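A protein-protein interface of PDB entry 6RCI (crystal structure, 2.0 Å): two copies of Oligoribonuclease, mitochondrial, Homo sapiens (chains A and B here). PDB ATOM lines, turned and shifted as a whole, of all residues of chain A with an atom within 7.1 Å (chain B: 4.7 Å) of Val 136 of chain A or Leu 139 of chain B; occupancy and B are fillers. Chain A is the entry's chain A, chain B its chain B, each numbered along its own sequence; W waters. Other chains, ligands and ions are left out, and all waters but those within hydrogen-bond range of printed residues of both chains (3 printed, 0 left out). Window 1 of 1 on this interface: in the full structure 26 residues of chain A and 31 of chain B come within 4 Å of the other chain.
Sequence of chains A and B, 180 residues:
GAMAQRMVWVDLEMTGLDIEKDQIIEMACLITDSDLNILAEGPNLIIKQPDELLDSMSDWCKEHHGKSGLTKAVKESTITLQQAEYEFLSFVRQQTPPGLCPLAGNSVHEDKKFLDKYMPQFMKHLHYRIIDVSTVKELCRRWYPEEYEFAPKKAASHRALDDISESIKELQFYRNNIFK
Val 136 of chain A touches Leu 139 of chain B, and with the chains exchanged Leu 139 of chain A touches Val 136 of chain B.
8 positions are printed for both chains.
The side-chain hydroxyl of Ser 134 of chain A sits at hydrogen-bond distance from the side-chain carboxylate of Asp 132 of chain A (2.7 Å).
The side-chain carboxylate of Glu 138 of chain B lies within salt-bridge range of the guanidinium group of Arg 141 of chain B (2.9 Å).
The guanidinium group of Arg 142 of chain B lies within salt-bridge range of the side-chain carboxylate of Glu 138 of chain B.
The side-chain hydroxyl of Ser 34 of chain A lies within hydrogen-bond range of the guanidinium group of Arg 142 of chain B.
The indole nitrogen (NE1) of Trp 143 of chain B is in hydrogen-bond range of the backbone carbonyl oxygen (O) of Ser 34 of chain A (2.9 Å).
N of Asp 132 of chain A lies within hydrogen-bond range of OG1 of Thr 135 of chain B (3.0 Å).
Of the printed residues of chain B, Met 7 of chain A touches Arg 142 (3.9 Å).
Of the printed residues of chain B, Leu 36 of chain A touches Trp 143 (3.7 Å).
Printed residues of chain B within 4 Å of Ile 131 of chain A: Thr 135, Glu 138 and Arg 142.
Val 136 of chain A touches one residue of chain B.
Of the printed residues of chain A, Thr 135 of chain B touches Ile 131 (3.9 Å) and Asp 132 (3.0 Å).
Printed residues of chain A within 4 Å of Leu 139 of chain B: Val 136 (3.7 Å).
Hydrophobic or aromatic side chains of chain A within 4 Å of the printed part of chain B: Met 7, Leu 36, Ile 131, Val 136, Leu 139 and Phe 179.
Of the 10 printed residues of chain B, 7 touch a printed residue of chain A.
Printed residues of chain B that touch a printed residue of chain A: Thr 135, Val 136, Glu 138, Leu 139, Arg 142, Trp 143 and Tyr 144.
Hydrophobic or aromatic side chains of chain B within 4 Å of the printed part of chain A: Val 136, Leu 139, Trp 143 and Tyr 144.
Among the printed residues, no Asp or Glu carboxylate lies within 4 Å of a Lys or Arg side-chain nitrogen of the other chain.
Among the printed residues, pairs that only touch across the chains: Phe 179 of chain A with Tyr 144 of chain B, Arg 175 of chain A with Trp 143 of chain B, Ile 131 of chain A with Arg 142 of chain B, Ile 131 of chain A with Glu 138 of chain B, Leu 139 of chain A with Val 136 of chain B, Val 136 of chain A with Leu 139 of chain B, Leu 36 of chain A with Trp 143 of chain B, Ile 131 of chain A with Thr 135 of chain B and Met 7 of chain A with Arg 142 of chain B.
Water W3 lies within hydrogen-bond range of the guanidinium group of Arg 175 of chain A (2.8 Å) and the backbone carbonyl oxygen of Trp 143 of chain B (2.8 Å).
Water W1 bridges the guanidinium group of Arg 175 of chain A (2.8 Å) and the side-chain hydroxyl of Tyr 144 of chain B (2.9 Å).
Water W2 bridges the side-chain hydroxyl (OG) of Ser 34 of chain A and the backbone carbonyl oxygen (O) of Arg 142 of chain B.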
ATOM      1  N   MET A   7       2.939   1.585  -7.318  1.00  0.00           N
ATOM      2  CA  MET A   7       2.762   0.210  -7.780  1.00  0.00           C
ATOM      3  C   MET A   7       3.751  -0.684  -7.106  1.00  0.00           C
ATOM      4  O   MET A   7       4.930  -0.330  -7.030  1.00  0.00           O
ATOM      5  CB  MET A   7       3.032   0.098  -9.289  1.00  0.00           C
ATOM      6  CG  MET A   7       1.994   0.753 -10.141  1.00  0.00           C
ATOM      7  SD  MET A   7       2.421   0.593 -11.920  1.00  0.00           S
ATOM      8  CE  MET A   7       1.694   2.009 -12.476  1.00  0.00           C
ATOM      9  N   SER A  34       3.003   6.040 -10.084  1.00  0.00           N
ATOM     10  CA  SER A  34       1.948   5.803 -11.078  1.00  0.00           C
ATOM     11  C   SER A  34       2.427   5.821 -12.553  1.00  0.00           C
ATOM     12  O   SER A  34       1.835   5.153 -13.398  1.00  0.00           O
ATOM     13  CB  SER A  34       0.840   6.837 -10.908  1.00  0.00           C
ATOM     14  OG  SER A  34      -0.354   6.438 -11.563  1.00  0.00           O
ATOM     15  N   LEU A  36       5.481   4.873 -13.645  1.00  0.00           N
ATOM     16  CA  LEU A  36       6.582   3.942 -13.861  1.00  0.00           C
ATOM     17  C   LEU A  36       7.974   4.512 -13.562  1.00  0.00           C
ATOM     18  O   LEU A  36       8.970   3.893 -13.958  1.00  0.00           O
ATOM     19  CB  LEU A  36       6.526   3.360 -15.306  1.00  0.00           C
ATOM     20  CG  LEU A  36       5.135   2.896 -15.790  1.00  0.00           C
ATOM     21  CD1 LEU A  36       5.235   2.231 -17.134  1.00  0.00           C
ATOM     22  CD2 LEU A  36       4.464   1.945 -14.753  1.00  0.00           C
ATOM     23  N   ILE A 131      -1.795  -5.139 -12.323  1.00  0.00           N
ATOM     24  CA  ILE A 131      -1.328  -4.521 -13.563  1.00  0.00           C
ATOM     25  C   ILE A 131      -0.451  -5.596 -14.181  1.00  0.00           C
ATOM     26  O   ILE A 131       0.560  -5.979 -13.595  1.00  0.00           O
ATOM     27  CB  ILE A 131      -0.589  -3.158 -13.363  1.00  0.00           C
ATOM     28  CG1 ILE A 131      -1.589  -2.088 -12.899  1.00  0.00           C
ATOM     29  CG2 ILE A 131       0.068  -2.724 -14.700  1.00  0.00           C
ATOM     30  CD1 ILE A 131      -0.978  -0.781 -12.311  1.00  0.00           C
ATOM     31  N   ASP A 132      -0.893  -6.171 -15.292  1.00  0.00           N
ATOM     32  CA  ASP A 132      -0.147  -7.251 -15.927  1.00  0.00           C
ATOM     33  C   ASP A 132       0.401  -6.767 -17.263  1.00  0.00           C
ATOM     34  O   ASP A 132      -0.343  -6.599 -18.233  1.00  0.00           O
ATOM     35  CB  ASP A 132      -1.016  -8.511 -16.081  1.00  0.00           C
ATOM     36  CG  ASP A 132      -0.193  -9.778 -16.325  1.00  0.00           C
ATOM     37  OD1 ASP A 132       0.802  -9.712 -17.092  1.00  0.00           O
ATOM     38  OD2 ASP A 132      -0.545 -10.838 -15.752  1.00  0.00           O
ATOM     39  N   VAL A 133       1.718  -6.642 -17.337  1.00  0.00           N
ATOM     40  CA  VAL A 133       2.398  -6.166 -18.555  1.00  0.00           C
ATOM     41  C   VAL A 133       2.120  -7.055 -19.732  1.00  0.00           C
ATOM     42  O   VAL A 133       2.089  -6.563 -20.855  1.00  0.00           O
ATOM     43  CB  VAL A 133       3.941  -5.976 -18.372  1.00  0.00           C
ATOM     44  CG1 VAL A 133       4.569  -5.433 -19.662  1.00  0.00           C
ATOM     45  CG2 VAL A 133       4.255  -5.072 -17.192  1.00  0.00           C
ATOM     46  N   SER A 134       1.939  -8.361 -19.500  1.00  0.00           N
ATOM     47  CA  SER A 134       1.687  -9.305 -20.582  1.00  0.00           C
ATOM     48  C   SER A 134       0.332  -9.077 -21.280  1.00  0.00           C
ATOM     49  O   SER A 134       0.228  -9.428 -22.431  1.00  0.00           O
ATOM     50  CB  SER A 134       1.855 -10.750 -20.089  1.00  0.00           C
ATOM     51  OG  SER A 134       0.722 -11.197 -19.366  1.00  0.00           O
ATOM     52  N   THR A 135      -0.708  -8.505 -20.602  1.00  0.00           N
ATOM     53  CA  THR A 135      -1.969  -8.170 -21.296  1.00  0.00           C
ATOM     54  C   THR A 135      -1.646  -7.100 -22.342  1.00  0.00           C
ATOM     55  O   THR A 135      -2.181  -7.158 -23.446  1.00  0.00           O
ATOM     56  CB  THR A 135      -2.996  -7.528 -20.350  1.00  0.00           C
ATOM     57  OG1 THR A 135      -3.587  -8.551 -19.556  1.00  0.00           O
ATOM     58  CG2 THR A 135      -4.087  -6.741 -21.100  1.00  0.00           C
ATOM     59  N   VAL A 136      -0.776  -6.097 -21.965  1.00  0.00           N
ATOM     60  CA  VAL A 136      -0.401  -5.004 -22.871  1.00  0.00           C
ATOM     61  C   VAL A 136       0.418  -5.570 -24.018  1.00  0.00           C
ATOM     62  O   VAL A 136       0.190  -5.171 -25.155  1.00  0.00           O
ATOM     63  CB  VAL A 136       0.286  -3.797 -22.167  1.00  0.00           C
ATOM     64  CG1 VAL A 136       0.407  -2.618 -23.121  1.00  0.00           C
ATOM     65  CG2 VAL A 136      -0.493  -3.381 -20.912  1.00  0.00           C
ATOM     66  N   LYS A 137       1.350  -6.506 -23.724  1.00  0.00           N
ATOM     67  CA  LYS A 137       2.149  -7.206 -24.727  1.00  0.00           C
ATOM     68  C   LYS A 137       1.250  -7.851 -25.797  1.00  0.00           C
ATOM     69  O   LYS A 137       1.533  -7.704 -26.981  1.00  0.00           O
ATOM     70  CB  LYS A 137       3.017  -8.302 -24.077  1.00  0.00           C
ATOM     71  CG  LYS A 137       3.971  -9.009 -25.077  1.00  0.00           C
ATOM     72  CD  LYS A 137       4.271 -10.465 -24.650  1.00  0.00           C
ATOM     73  CE  LYS A 137       5.421 -11.173 -25.371  1.00  0.00           C
ATOM     74  NZ  LYS A 137       6.579 -10.299 -25.753  1.00  0.00           N
ATOM     75  N   GLU A 138       0.211  -8.597 -25.382  1.00  0.00           N
ATOM     76  CA  GLU A 138      -0.715  -9.279 -26.336  1.00  0.00           C
ATOM     77  C   GLU A 138      -1.481  -8.297 -27.213  1.00  0.00           C
ATOM     78  O   GLU A 138      -1.633  -8.541 -28.401  1.00  0.00           O
ATOM     79  CB  GLU A 138      -1.701 -10.209 -25.589  1.00  0.00           C
ATOM     80  CG  GLU A 138      -1.043 -11.461 -25.011  1.00  0.00           C
ATOM     81  CD  GLU A 138      -0.366 -12.346 -26.039  1.00  0.00           C
ATOM     82  OE1 GLU A 138      -1.022 -12.708 -27.037  1.00  0.00           O
ATOM     83  OE2 GLU A 138       0.832 -12.649 -25.875  1.00  0.00           O
ATOM     84  N   LEU A 139      -1.931  -7.184 -26.640  1.00  0.00           N
ATOM     85  CA  LEU A 139      -2.614  -6.134 -27.391  1.00  0.00           C
ATOM     86  C   LEU A 139      -1.615  -5.394 -28.324  1.00  0.00           C
ATOM     87  O   LEU A 139      -1.975  -5.053 -29.449  1.00  0.00           O
ATOM     88  CB  LEU A 139      -3.299  -5.152 -26.432  1.00  0.00           C
ATOM     89  CG  LEU A 139      -4.369  -5.728 -25.514  1.00  0.00           C
ATOM     90  CD1 LEU A 139      -4.876  -4.666 -24.558  1.00  0.00           C
ATOM     91  CD2 LEU A 139      -5.501  -6.358 -26.297  1.00  0.00           C
ATOM     92  N   CYS A 140      -0.364  -5.194 -27.902  1.00  0.00           N
ATOM     93  CA  CYS A 140       0.643  -4.547 -28.764  1.00  0.00           C
ATOM     94  C   CYS A 140       0.914  -5.378 -29.997  1.00  0.00           C
ATOM     95  O   CYS A 140       0.984  -4.835 -31.090  1.00  0.00           O
ATOM     96  CB  CYS A 140       1.943  -4.286 -28.010  1.00  0.00           C
ATOM     97  SG  CYS A 140       3.155  -3.311 -28.948  1.00  0.00           S
ATOM     98  N   ARG A 141       1.083  -6.688 -29.822  1.00  0.00           N
ATOM     99  CA  ARG A 141       1.368  -7.609 -30.923  1.00  0.00           C
ATOM    100  C   ARG A 141       0.254  -7.605 -31.978  1.00  0.00           C
ATOM    101  O   ARG A 141       0.533  -7.716 -33.177  1.00  0.00           O
ATOM    102  CB  ARG A 141       1.572  -9.050 -30.389  1.00  0.00           C
ATOM    103  CG  ARG A 141       2.250  -9.947 -31.419  1.00  0.00           C
ATOM    104  CD  ARG A 141       2.815 -11.268 -30.891  1.00  0.00           C
ATOM    105  NE  ARG A 141       1.919 -12.383 -31.196  1.00  0.00           N
ATOM    106  CZ  ARG A 141       0.922 -12.801 -30.425  1.00  0.00           C
ATOM    107  NH1 ARG A 141       0.690 -12.225 -29.251  1.00  0.00           N
ATOM    108  NH2 ARG A 141       0.154 -13.814 -30.815  1.00  0.00           N
ATOM    109  N   ARG A 142      -0.983  -7.483 -31.536  1.00  0.00           N
ATOM    110  CA  ARG A 142      -2.138  -7.474 -32.434  1.00  0.00           C
ATOM    111  C   ARG A 142      -2.374  -6.114 -33.067  1.00  0.00           C
ATOM    112  O   ARG A 142      -2.445  -5.989 -34.285  1.00  0.00           O
ATOM    113  CB  ARG A 142      -3.406  -7.856 -31.659  1.00  0.00           C
ATOM    114  CG  ARG A 142      -3.402  -9.310 -31.225  1.00  0.00           C
ATOM    115  CD  ARG A 142      -4.421  -9.558 -30.136  1.00  0.00           C
ATOM    116  NE  ARG A 142      -4.660 -10.987 -29.969  1.00  0.00           N
ATOM    117  CZ  ARG A 142      -3.851 -11.835 -29.347  1.00  0.00           C
ATOM    118  NH1 ARG A 142      -2.716 -11.410 -28.803  1.00  0.00           N
ATOM    119  NH2 ARG A 142      -4.163 -13.123 -29.270  1.00  0.00           N
ATOM    120  N   TYR A 148       5.618  -3.385 -31.984  1.00  0.00           N
ATOM    121  CA  TYR A 148       5.988  -4.640 -31.321  1.00  0.00           C
ATOM    122  C   TYR A 148       7.351  -5.163 -31.804  1.00  0.00           C
ATOM    123  O   TYR A 148       8.111  -5.710 -31.008  1.00  0.00           O
ATOM    124  CB  TYR A 148       4.950  -5.717 -31.582  1.00  0.00           C
ATOM    125  CG  TYR A 148       5.152  -6.959 -30.752  1.00  0.00           C
ATOM    126  CD1 TYR A 148       4.927  -6.943 -29.381  1.00  0.00           C
ATOM    127  CD2 TYR A 148       5.494  -8.172 -31.344  1.00  0.00           C
ATOM    128  CE1 TYR A 148       5.085  -8.089 -28.609  1.00  0.00           C
ATOM    129  CE2 TYR A 148       5.592  -9.343 -30.588  1.00  0.00           C
ATOM    130  CZ  TYR A 148       5.369  -9.297 -29.220  1.00  0.00           C
ATOM    131  OH  TYR A 148       5.437 -10.412 -28.426  1.00  0.00           O
ATOM    132  N   GLU A 170       9.613  -2.910 -20.264  1.00  0.00           N
ATOM    133  CA  GLU A 170       8.625  -3.324 -21.259  1.00  0.00           C
ATOM    134  C   GLU A 170       7.351  -2.495 -21.196  1.00  0.00           C
ATOM    135  O   GLU A 170       6.854  -2.086 -22.239  1.00  0.00           O
ATOM    136  CB  GLU A 170       8.304  -4.807 -21.083  1.00  0.00           C
ATOM    137  CG  GLU A 170       7.401  -5.336 -22.184  1.00  0.00           C
ATOM    138  CD  GLU A 170       6.914  -6.759 -22.019  1.00  0.00           C
ATOM    139  OE1 GLU A 170       7.258  -7.418 -21.011  1.00  0.00           O
ATOM    140  OE2 GLU A 170       6.150  -7.205 -22.901  1.00  0.00           O
ATOM    141  N   LEU A 171       6.809  -2.219 -19.981  1.00  0.00           N
ATOM    142  CA  LEU A 171       5.583  -1.427 -19.913  1.00  0.00           C
ATOM    143  C   LEU A 171       5.846   0.043 -20.260  1.00  0.00           C
ATOM    144  O   LEU A 171       4.987   0.680 -20.881  1.00  0.00           O
ATOM    145  CB  LEU A 171       4.919  -1.551 -18.541  1.00  0.00           C
ATOM    146  CG  LEU A 171       3.515  -0.898 -18.463  1.00  0.00           C
ATOM    147  CD1 LEU A 171       2.529  -1.561 -19.456  1.00  0.00           C
ATOM    148  CD2 LEU A 171       2.967  -0.956 -17.019  1.00  0.00           C
ATOM    149  N   TYR A 174       5.708   0.308 -23.946  1.00  0.00           N
ATOM    150  CA  TYR A 174       4.313   0.390 -24.414  1.00  0.00           C
ATOM    151  C   TYR A 174       3.726   1.751 -24.210  1.00  0.00           C
ATOM    152  O   TYR A 174       3.107   2.289 -25.135  1.00  0.00           O
ATOM    153  CB  TYR A 174       3.407  -0.690 -23.790  1.00  0.00           C
ATOM    154  CG  TYR A 174       3.841  -2.093 -24.127  1.00  0.00           C
ATOM    155  CD1 TYR A 174       4.271  -2.424 -25.415  1.00  0.00           C
ATOM    156  CD2 TYR A 174       3.813  -3.100 -23.170  1.00  0.00           C
ATOM    157  CE1 TYR A 174       4.780  -3.686 -25.700  1.00  0.00           C
ATOM    158  CE2 TYR A 174       4.232  -4.394 -23.474  1.00  0.00           C
ATOM    159  CZ  TYR A 174       4.779  -4.661 -24.720  1.00  0.00           C
ATOM    160  OH  TYR A 174       5.317  -5.886 -25.017  1.00  0.00           O
ATOM    161  N   ARG A 175       3.919   2.339 -23.033  1.00  0.00           N
ATOM    162  CA  ARG A 175       3.397   3.685 -22.792  1.00  0.00           C
ATOM    163  C   ARG A 175       3.982   4.670 -23.804  1.00  0.00           C
ATOM    164  O   ARG A 175       3.253   5.471 -24.397  1.00  0.00           O
ATOM    165  CB  ARG A 175       3.716   4.190 -21.380  1.00  0.00           C
ATOM    166  CG  ARG A 175       2.833   5.388 -21.109  1.00  0.00           C
ATOM    167  CD  ARG A 175       3.133   6.156 -19.870  1.00  0.00           C
ATOM    168  NE  ARG A 175       2.117   7.208 -19.726  1.00  0.00           N
ATOM    169  CZ  ARG A 175       1.939   7.945 -18.635  1.00  0.00           C
ATOM    170  NH1 ARG A 175       2.710   7.766 -17.572  1.00  0.00           N
ATOM    171  NH2 ARG A 175       0.984   8.868 -18.598  1.00  0.00           N
ATOM    172  N   ILE A 178       2.640   3.046 -27.855  1.00  0.00           N
ATOM    173  CA  ILE A 178       1.296   2.629 -28.348  1.00  0.00           C
ATOM    174  C   ILE A 178       0.136   3.300 -27.609  1.00  0.00           C
ATOM    175  O   ILE A 178      -1.018   3.085 -28.005  1.00  0.00           O
ATOM    176  CB  ILE A 178       1.123   1.060 -28.384  1.00  0.00           C
ATOM    177  CG1 ILE A 178       1.032   0.437 -26.977  1.00  0.00           C
ATOM    178  CG2 ILE A 178       2.274   0.412 -29.184  1.00  0.00           C
ATOM    179  CD1 ILE A 178       0.666  -0.988 -27.009  1.00  0.00           C
ATOM    180  N   PHE A 179       0.417   4.100 -26.579  1.00  0.00           N
ATOM    181  CA  PHE A 179      -0.604   4.847 -25.870  1.00  0.00           C
ATOM    182  C   PHE A 179      -0.614   6.257 -26.492  1.00  0.00           C
ATOM    183  O   PHE A 179       0.416   6.750 -26.976  1.00  0.00           O
ATOM    184  CB  PHE A 179      -0.358   4.823 -24.337  1.00  0.00           C
ATOM    185  CG  PHE A 179      -0.797   3.527 -23.685  1.00  0.00           C
ATOM    186  CD1 PHE A 179      -2.095   3.376 -23.206  1.00  0.00           C
ATOM    187  CD2 PHE A 179       0.020   2.402 -23.723  1.00  0.00           C
ATOM    188  CE1 PHE A 179      -2.519   2.161 -22.663  1.00  0.00           C
ATOM    189  CE2 PHE A 179      -0.408   1.183 -23.190  1.00  0.00           C
ATOM    190  CZ  PHE A 179      -1.663   1.079 -22.635  1.00  0.00           C
ATOM    191  N   THR B 135      -6.454  -4.824 -16.400  1.00  0.00           N
ATOM    192  CA  THR B 135      -5.137  -4.189 -16.502  1.00  0.00           C
ATOM    193  C   THR B 135      -5.296  -2.874 -17.282  1.00  0.00           C
ATOM    194  O   THR B 135      -4.752  -1.859 -16.868  1.00  0.00           O
ATOM    195  CB  THR B 135      -4.127  -5.110 -17.227  1.00  0.00           C
ATOM    196  OG1 THR B 135      -3.693  -6.136 -16.328  1.00  0.00           O
ATOM    197  CG2 THR B 135      -2.882  -4.340 -17.739  1.00  0.00           C
ATOM    198  N   VAL B 136      -6.054  -2.908 -18.424  1.00  0.00           N
ATOM    199  CA  VAL B 136      -6.218  -1.725 -19.275  1.00  0.00           C
ATOM    200  C   VAL B 136      -7.008  -0.657 -18.540  1.00  0.00           C
ATOM    201  O   VAL B 136      -6.657   0.522 -18.618  1.00  0.00           O
ATOM    202  CB  VAL B 136      -6.793  -2.079 -20.688  1.00  0.00           C
ATOM    203  CG1 VAL B 136      -6.780  -0.851 -21.607  1.00  0.00           C
ATOM    204  CG2 VAL B 136      -5.992  -3.225 -21.342  1.00  0.00           C
ATOM    205  N   LYS B 137      -8.044  -1.059 -17.791  1.00  0.00           N
ATOM    206  CA  LYS B 137      -8.860  -0.125 -17.003  1.00  0.00           C
ATOM    207  C   LYS B 137      -7.986   0.658 -16.049  1.00  0.00           C
ATOM    208  O   LYS B 137      -8.127   1.871 -15.911  1.00  0.00           O
ATOM    209  CB  LYS B 137      -9.954  -0.885 -16.190  1.00  0.00           C
ATOM    210  CG  LYS B 137     -10.833   0.055 -15.331  1.00  0.00           C
ATOM    211  CD  LYS B 137     -12.030  -0.628 -14.696  1.00  0.00           C
ATOM    212  CE  LYS B 137     -13.101   0.313 -14.162  1.00  0.00           C
ATOM    213  NZ  LYS B 137     -13.241   0.256 -12.684  1.00  0.00           N
ATOM    214  N   GLU B 138      -7.082  -0.055 -15.385  1.00  0.00           N
ATOM    215  CA  GLU B 138      -6.194   0.510 -14.398  1.00  0.00           C
ATOM    216  C   GLU B 138      -5.184   1.473 -15.001  1.00  0.00           C
ATOM    217  O   GLU B 138      -4.917   2.510 -14.404  1.00  0.00           O
ATOM    218  CB  GLU B 138      -5.547  -0.653 -13.623  1.00  0.00           C
ATOM    219  CG  GLU B 138      -4.732  -0.260 -12.429  1.00  0.00           C
ATOM    220  CD  GLU B 138      -5.329   0.710 -11.428  1.00  0.00           C
ATOM    221  OE1 GLU B 138      -6.564   0.895 -11.396  1.00  0.00           O
ATOM    222  OE2 GLU B 138      -4.540   1.279 -10.644  1.00  0.00           O
ATOM    223  N   LEU B 139      -4.664   1.169 -16.217  1.00  0.00           N
ATOM    224  CA  LEU B 139      -3.770   2.072 -16.910  1.00  0.00           C
ATOM    225  C   LEU B 139      -4.565   3.277 -17.388  1.00  0.00           C
ATOM    226  O   LEU B 139      -4.049   4.387 -17.316  1.00  0.00           O
ATOM    227  CB  LEU B 139      -3.068   1.360 -18.074  1.00  0.00           C
ATOM    228  CG  LEU B 139      -2.133   0.205 -17.667  1.00  0.00           C
ATOM    229  CD1 LEU B 139      -1.468  -0.388 -18.879  1.00  0.00           C
ATOM    230  CD2 LEU B 139      -1.122   0.636 -16.604  1.00  0.00           C
ATOM    231  N   CYS B 140      -5.844   3.082 -17.818  1.00  0.00           N
ATOM    232  CA  CYS B 140      -6.720   4.195 -18.198  1.00  0.00           C
ATOM    233  C   CYS B 140      -6.898   5.137 -17.006  1.00  0.00           C
ATOM    234  O   CYS B 140      -6.711   6.363 -17.118  1.00  0.00           O
ATOM    235  CB  CYS B 140      -8.074   3.683 -18.694  1.00  0.00           C
ATOM    236  SG  CYS B 140      -9.176   4.985 -19.300  1.00  0.00           S
ATOM    237  N   ARG B 141      -7.266   4.557 -15.856  1.00  0.00           N
ATOM    238  CA  ARG B 141      -7.488   5.320 -14.624  1.00  0.00           C
ATOM    239  C   ARG B 141      -6.315   6.224 -14.278  1.00  0.00           C
ATOM    240  O   ARG B 141      -6.533   7.402 -13.981  1.00  0.00           O
ATOM    241  CB  ARG B 141      -7.800   4.382 -13.439  1.00  0.00           C
ATOM    242  CG  ARG B 141      -8.338   5.146 -12.232  1.00  0.00           C
ATOM    243  CD  ARG B 141      -8.539   4.261 -11.010  1.00  0.00           C
ATOM    244  NE  ARG B 141      -7.276   3.738 -10.497  1.00  0.00           N
ATOM    245  CZ  ARG B 141      -6.381   4.416  -9.781  1.00  0.00           C
ATOM    246  NH1 ARG B 141      -6.585   5.691  -9.478  1.00  0.00           N
ATOM    247  NH2 ARG B 141      -5.267   3.825  -9.371  1.00  0.00           N
ATOM    248  N   ARG B 142      -5.068   5.692 -14.356  1.00  0.00           N
ATOM    249  CA  ARG B 142      -3.866   6.451 -13.997  1.00  0.00           C
ATOM    250  C   ARG B 142      -3.436   7.448 -15.052  1.00  0.00           C
ATOM    251  O   ARG B 142      -3.168   8.610 -14.748  1.00  0.00           O
ATOM    252  CB  ARG B 142      -2.672   5.484 -13.777  1.00  0.00           C
ATOM    253  CG  ARG B 142      -2.886   4.569 -12.597  1.00  0.00           C
ATOM    254  CD  ARG B 142      -2.027   3.308 -12.665  1.00  0.00           C
ATOM    255  NE  ARG B 142      -2.281   2.519 -11.461  1.00  0.00           N
ATOM    256  CZ  ARG B 142      -1.793   2.783 -10.259  1.00  0.00           C
ATOM    257  NH1 ARG B 142      -0.936   3.786 -10.085  1.00  0.00           N
ATOM    258  NH2 ARG B 142      -2.139   2.034  -9.218  1.00  0.00           N
ATOM    259  N   TRP B 143      -3.240   6.952 -16.261  1.00  0.00           N
ATOM    260  CA  TRP B 143      -2.652   7.739 -17.334  1.00  0.00           C
ATOM    261  C   TRP B 143      -3.641   8.596 -18.121  1.00  0.00           C
ATOM    262  O   TRP B 143      -3.203   9.550 -18.742  1.00  0.00           O
ATOM    263  CB  TRP B 143      -1.869   6.813 -18.269  1.00  0.00           C
ATOM    264  CG  TRP B 143      -0.809   5.990 -17.584  1.00  0.00           C
ATOM    265  CD1 TRP B 143      -0.182   6.264 -16.401  1.00  0.00           C
ATOM    266  CD2 TRP B 143      -0.168   4.822 -18.114  1.00  0.00           C
ATOM    267  NE1 TRP B 143       0.707   5.255 -16.097  1.00  0.00           N
ATOM    268  CE2 TRP B 143       0.805   4.413 -17.171  1.00  0.00           C
ATOM    269  CE3 TRP B 143      -0.251   4.136 -19.342  1.00  0.00           C
ATOM    270  CZ2 TRP B 143       1.659   3.327 -17.398  1.00  0.00           C
ATOM    271  CZ3 TRP B 143       0.514   2.991 -19.517  1.00  0.00           C
ATOM    272  CH2 TRP B 143       1.481   2.616 -18.570  1.00  0.00           C
ATOM    273  N   TYR B 144      -4.953   8.271 -18.094  1.00  0.00           N
ATOM    274  CA  TYR B 144      -6.005   8.968 -18.858  1.00  0.00           C
ATOM    275  C   TYR B 144      -7.210   9.244 -17.950  1.00  0.00           C
ATOM    276  O   TYR B 144      -8.284   8.700 -18.180  1.00  0.00           O
ATOM    277  CB  TYR B 144      -6.390   8.093 -20.053  1.00  0.00           C
ATOM    278  CG  TYR B 144      -5.197   7.939 -20.974  1.00  0.00           C
ATOM    279  CD1 TYR B 144      -4.854   8.946 -21.874  1.00  0.00           C
ATOM    280  CD2 TYR B 144      -4.334   6.853 -20.850  1.00  0.00           C
ATOM    281  CE1 TYR B 144      -3.704   8.865 -22.650  1.00  0.00           C
ATOM    282  CE2 TYR B 144      -3.173   6.764 -21.615  1.00  0.00           C
ATOM    283  CZ  TYR B 144      -2.841   7.793 -22.484  1.00  0.00           C
ATOM    284  OH  TYR B 144      -1.687   7.719 -23.222  1.00  0.00           O
HETATM  285  O   HOH W   1       0.899   8.242 -22.023  1.00  0.00           O
HETATM  286  O   HOH W   2      -0.197   8.421 -13.544  1.00  0.00           O
HETATM  287  O   HOH W   3      -0.940   9.842 -20.324  1.00  0.00           O
